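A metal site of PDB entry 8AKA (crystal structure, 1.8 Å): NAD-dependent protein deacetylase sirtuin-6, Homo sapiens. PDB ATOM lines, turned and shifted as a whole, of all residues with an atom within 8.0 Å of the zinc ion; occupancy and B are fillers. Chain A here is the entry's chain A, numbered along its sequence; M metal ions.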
ATOM      1  N   GLU A 134      16.529  11.747   6.886  1.00  0.00           N
ATOM      2  CA  GLU A 134      17.684  12.412   6.238  1.00  0.00           C
ATOM      3  C   GLU A 134      17.203  13.150   4.983  1.00  0.00           C
ATOM      4  O   GLU A 134      16.381  12.572   4.216  1.00  0.00           O
ATOM      5  CB  GLU A 134      18.747  11.361   5.928  1.00  0.00           C
ATOM      6  CG  GLU A 134      19.985  11.904   5.225  1.00  0.00           C
ATOM      7  CD  GLU A 134      21.071  10.865   5.053  1.00  0.00           C
ATOM      8  OE1 GLU A 134      21.794  10.616   6.030  1.00  0.00           O
ATOM      9  OE2 GLU A 134      21.185  10.301   3.958  1.00  0.00           O
ATOM     10  N   CYS A 135      17.685  14.372   4.788  1.00  0.00           N
ATOM     11  CA  CYS A 135      17.329  15.210   3.608  1.00  0.00           C
ATOM     12  C   CYS A 135      18.087  14.668   2.396  1.00  0.00           C
ATOM     13  O   CYS A 135      19.328  14.540   2.470  1.00  0.00           O
ATOM     14  CB  CYS A 135      17.687  16.668   3.837  1.00  0.00           C
ATOM     15  SG  CYS A 135      17.357  17.710   2.381  1.00  0.00           S
ATOM     16  N   ALA A 136      17.362  14.328   1.328  1.00  0.00           N
ATOM     17  CA  ALA A 136      17.998  13.842   0.082  1.00  0.00           C
ATOM     18  C   ALA A 136      18.946  14.905  -0.473  1.00  0.00           C
ATOM     19  O   ALA A 136      20.006  14.528  -0.966  1.00  0.00           O
ATOM     20  CB  ALA A 136      16.933  13.475  -0.913  1.00  0.00           C
ATOM     21  N   LYS A 137      18.593  16.184  -0.371  1.00  0.00           N
ATOM     22  CA  LYS A 137      19.410  17.288  -0.947  1.00  0.00           C
ATOM     23  C   LYS A 137      20.673  17.524  -0.130  1.00  0.00           C
ATOM     24  O   LYS A 137      21.761  17.349  -0.715  1.00  0.00           O
ATOM     25  CB  LYS A 137      18.601  18.582  -1.052  1.00  0.00           C
ATOM     26  CG  LYS A 137      17.438  18.533  -2.042  1.00  0.00           C
ATOM     27  CD  LYS A 137      16.864  19.888  -2.326  1.00  0.00           C
ATOM     28  CE  LYS A 137      15.812  19.876  -3.416  1.00  0.00           C
ATOM     29  NZ  LYS A 137      15.210  21.213  -3.596  1.00  0.00           N
ATOM     30  N   CYS A 138      20.557  17.897   1.158  1.00  0.00           N
ATOM     31  CA  CYS A 138      21.737  18.377   1.954  1.00  0.00           C
ATOM     32  C   CYS A 138      22.236  17.323   2.939  1.00  0.00           C
ATOM     33  O   CYS A 138      23.229  17.618   3.638  1.00  0.00           O
ATOM     34  CB  CYS A 138      21.434  19.678   2.684  1.00  0.00           C
ATOM     35  SG  CYS A 138      20.262  19.522   4.054  1.00  0.00           S
ATOM     36  N   LYS A 139      21.580  16.159   3.022  1.00  0.00           N
ATOM     37  CA  LYS A 139      22.032  15.016   3.878  1.00  0.00           C
ATOM     38  C   LYS A 139      21.895  15.405   5.349  1.00  0.00           C
ATOM     39  O   LYS A 139      22.486  14.708   6.184  1.00  0.00           O
ATOM     40  CB  LYS A 139      23.466  14.612   3.515  1.00  0.00           C
ATOM     41  CG  LYS A 139      23.723  14.376   2.028  1.00  0.00           C
ATOM     42  CD  LYS A 139      22.870  13.280   1.417  1.00  0.00           C
ATOM     43  CE  LYS A 139      23.218  13.038  -0.042  1.00  0.00           C
ATOM     44  NZ  LYS A 139      22.395  11.960  -0.624  1.00  0.00           N
ATOM     45  N   THR A 140      21.110  16.436   5.667  1.00  0.00           N
ATOM     46  CA  THR A 140      20.905  16.841   7.080  1.00  0.00           C
ATOM     47  C   THR A 140      20.011  15.776   7.714  1.00  0.00           C
ATOM     48  O   THR A 140      18.931  15.517   7.170  1.00  0.00           O
ATOM     49  CB  THR A 140      20.342  18.250   7.224  1.00  0.00           C
ATOM     50  OG1 THR A 140      21.352  19.157   6.792  1.00  0.00           O
ATOM     51  CG2 THR A 140      19.944  18.565   8.656  1.00  0.00           C
ATOM     52  N   GLN A 141      20.483  15.180   8.804  1.00  0.00           N
ATOM     53  CA  GLN A 141      19.723  14.169   9.582  1.00  0.00           C
ATOM     54  C   GLN A 141      18.908  14.845  10.678  1.00  0.00           C
ATOM     55  O   GLN A 141      19.300  15.940  11.189  1.00  0.00           O
ATOM     56  CB  GLN A 141      20.657  13.096  10.124  1.00  0.00           C
ATOM     57  CG  GLN A 141      21.246  12.274   9.004  1.00  0.00           C
ATOM     58  CD  GLN A 141      22.051  11.121   9.514  1.00  0.00           C
ATOM     59  OE1 GLN A 141      22.689  11.207  10.563  1.00  0.00           O
ATOM     60  NE2 GLN A 141      22.025  10.022   8.773  1.00  0.00           N
ATOM     61  N   TYR A 142      17.782  14.230  11.002  1.00  0.00           N
ATOM     62  CA  TYR A 142      16.835  14.676  12.041  1.00  0.00           C
ATOM     63  C   TYR A 142      16.558  13.454  12.906  1.00  0.00           C
ATOM     64  O   TYR A 142      16.144  12.394  12.325  1.00  0.00           O
ATOM     65  CB  TYR A 142      15.548  15.233  11.401  1.00  0.00           C
ATOM     66  CG  TYR A 142      15.731  16.446  10.528  1.00  0.00           C
ATOM     67  CD1 TYR A 142      16.181  16.333   9.226  1.00  0.00           C
ATOM     68  CD2 TYR A 142      15.405  17.698  11.016  1.00  0.00           C
ATOM     69  CE1 TYR A 142      16.352  17.464   8.433  1.00  0.00           C
ATOM     70  CE2 TYR A 142      15.539  18.841  10.239  1.00  0.00           C
ATOM     71  CZ  TYR A 142      16.026  18.722   8.937  1.00  0.00           C
ATOM     72  OH  TYR A 142      16.160  19.857   8.194  1.00  0.00           O
ATOM     73  N   LEU A 159       9.719  17.733   5.178  1.00  0.00           N
ATOM     74  CA  LEU A 159      10.671  18.538   4.360  1.00  0.00           C
ATOM     75  C   LEU A 159      11.761  19.129   5.254  1.00  0.00           C
ATOM     76  O   LEU A 159      11.500  19.415   6.444  1.00  0.00           O
ATOM     77  CB  LEU A 159       9.902  19.628   3.611  1.00  0.00           C
ATOM     78  CG  LEU A 159       8.833  19.120   2.643  1.00  0.00           C
ATOM     79  CD1 LEU A 159       8.126  20.292   1.968  1.00  0.00           C
ATOM     80  CD2 LEU A 159       9.422  18.176   1.599  1.00  0.00           C
ATOM     81  N   CYS A 160      12.954  19.273   4.684  1.00  0.00           N
ATOM     82  CA  CYS A 160      14.149  19.880   5.300  1.00  0.00           C
ATOM     83  C   CYS A 160      13.838  21.320   5.746  1.00  0.00           C
ATOM     84  O   CYS A 160      13.218  22.055   4.953  1.00  0.00           O
ATOM     85  CB  CYS A 160      15.276  19.884   4.285  1.00  0.00           C
ATOM     86  SG  CYS A 160      16.911  19.993   5.042  1.00  0.00           S
ATOM     87  N   THR A 161      14.242  21.678   6.967  1.00  0.00           N
ATOM     88  CA  THR A 161      14.041  23.020   7.578  1.00  0.00           C
ATOM     89  C   THR A 161      15.380  23.761   7.701  1.00  0.00           C
ATOM     90  O   THR A 161      15.404  24.781   8.389  1.00  0.00           O
ATOM     91  CB  THR A 161      13.338  22.902   8.938  1.00  0.00           C
ATOM     92  OG1 THR A 161      14.227  22.271   9.862  1.00  0.00           O
ATOM     93  CG2 THR A 161      12.040  22.130   8.875  1.00  0.00           C
ATOM     94  N   VAL A 162      16.456  23.287   7.060  1.00  0.00           N
ATOM     95  CA  VAL A 162      17.771  23.998   7.129  1.00  0.00           C
ATOM     96  C   VAL A 162      17.588  25.353   6.428  1.00  0.00           C
ATOM     97  O   VAL A 162      16.966  25.370   5.348  1.00  0.00           O
ATOM     98  CB  VAL A 162      18.957  23.191   6.551  1.00  0.00           C
ATOM     99  CG1 VAL A 162      20.242  24.004   6.567  1.00  0.00           C
ATOM    100  CG2 VAL A 162      19.152  21.880   7.289  1.00  0.00           C
ATOM    101  N   ALA A 163      18.100  26.427   7.047  1.00  0.00           N
ATOM    102  CA  ALA A 163      17.836  27.848   6.682  1.00  0.00           C
ATOM    103  C   ALA A 163      18.065  28.067   5.181  1.00  0.00           C
ATOM    104  O   ALA A 163      19.244  28.067   4.773  1.00  0.00           O
ATOM    105  CB  ALA A 163      18.712  28.748   7.517  1.00  0.00           C
ATOM    106  N   CYS A 171      15.758  24.949   2.289  1.00  0.00           N
ATOM    107  CA  CYS A 171      16.094  23.706   1.552  1.00  0.00           C
ATOM    108  C   CYS A 171      14.816  23.014   1.077  1.00  0.00           C
ATOM    109  O   CYS A 171      14.729  22.677  -0.118  1.00  0.00           O
ATOM    110  CB  CYS A 171      16.884  22.742   2.435  1.00  0.00           C
ATOM    111  SG  CYS A 171      17.321  21.206   1.587  1.00  0.00           S
ATOM    112  N   ARG A 172      13.875  22.787   1.991  1.00  0.00           N
ATOM    113  CA  ARG A 172      12.606  22.068   1.722  1.00  0.00           C
ATOM    114  C   ARG A 172      12.902  20.757   0.984  1.00  0.00           C
ATOM    115  O   ARG A 172      12.013  20.239   0.278  1.00  0.00           O
ATOM    116  CB  ARG A 172      11.626  22.953   0.941  1.00  0.00           C
ATOM    117  CG  ARG A 172      11.407  24.322   1.561  1.00  0.00           C
ATOM    118  CD  ARG A 172      10.067  24.950   1.202  1.00  0.00           C
ATOM    119  NE  ARG A 172       9.566  24.530  -0.111  1.00  0.00           N
ATOM    120  CZ  ARG A 172       8.536  23.705  -0.340  1.00  0.00           C
ATOM    121  NH1 ARG A 172       7.836  23.207   0.664  1.00  0.00           N
ATOM    122  NH2 ARG A 172       8.200  23.402  -1.582  1.00  0.00           N
ATOM    123  N   GLY A 173      14.102  20.202   1.184  1.00  0.00           N
ATOM    124  CA  GLY A 173      14.500  18.892   0.627  1.00  0.00           C
ATOM    125  C   GLY A 173      13.616  17.785   1.178  1.00  0.00           C
ATOM    126  O   GLY A 173      13.196  17.870   2.351  1.00  0.00           O
ATOM    127  N   GLU A 174      13.288  16.813   0.316  1.00  0.00           N
ATOM    128  CA  GLU A 174      12.560  15.588   0.661  1.00  0.00           C
ATOM    129  C   GLU A 174      13.296  14.876   1.806  1.00  0.00           C
ATOM    130  O   GLU A 174      14.501  14.576   1.629  1.00  0.00           O
ATOM    131  CB  GLU A 174      12.448  14.703  -0.591  1.00  0.00           C
ATOM    132  CG  GLU A 174      11.453  13.571  -0.467  1.00  0.00           C
ATOM    133  CD  GLU A 174      11.121  12.919  -1.808  1.00  0.00           C
ATOM    134  OE1 GLU A 174      10.513  13.617  -2.655  1.00  0.00           O
ATOM    135  OE2 GLU A 174      11.476  11.736  -2.008  1.00  0.00           O
ATOM    136  N   LEU A 175      12.620  14.661   2.935  1.00  0.00           N
ATOM    137  CA  LEU A 175      13.127  13.806   4.042  1.00  0.00           C
ATOM    138  C   LEU A 175      12.735  12.353   3.776  1.00  0.00           C
ATOM    139  O   LEU A 175      11.577  12.089   3.390  1.00  0.00           O
ATOM    140  CB  LEU A 175      12.586  14.279   5.394  1.00  0.00           C
ATOM    141  CG  LEU A 175      12.987  15.700   5.798  1.00  0.00           C
ATOM    142  CD1 LEU A 175      12.601  15.942   7.242  1.00  0.00           C
ATOM    143  CD2 LEU A 175      14.465  15.940   5.576  1.00  0.00           C
HETATM  144 ZN    ZN M   1      18.180  19.730   3.220  1.00  0.00          ZN
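The zinc ion is bound by the side-chain sulfur of Cys 160 (2.2 Å), the side-chain sulfur of Cys 138 (2.3 Å), the side-chain sulfur of Cys 135 (2.3 Å) and the side-chain sulfur of Cys 171 (2.4 Å).
The zinc ion has four donor atoms within binding distance.
Of the 19 residues printed, 4 come within 4 Å of the zinc ion.
The backbone NH of Gly 173 sits close to the side-chain sulfur of Cys 171, at 3.4 Å.
The side-chain sulfur (SG) of Cys 138 sits close to the side-chain hydroxyl (OG1) of Thr 140, 3.0 Å away.
The backbone NH of Cys 160 sits at hydrogen-bond distance from the backbone carbonyl oxygen of Gly 173, at 2.7 Å.
O of Thr 140 lies within hydrogen-bond range of N of Cys 135 (2.9 Å).
The backbone carbonyl oxygen (O) of Cys 160 lies within hydrogen-bond range of the backbone NH (N) of Arg 172 (3.1 Å).
SG of Cys 135 lies close to N of Lys 137 (3.4 Å).
N of Cys 171 lies within hydrogen-bond range of O of Val 162 (3.3 Å).
The side-chain sulfur (SG) of Cys 160 sits close to the side-chain hydroxyl (OH) of Tyr 142 (3.2 Å).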
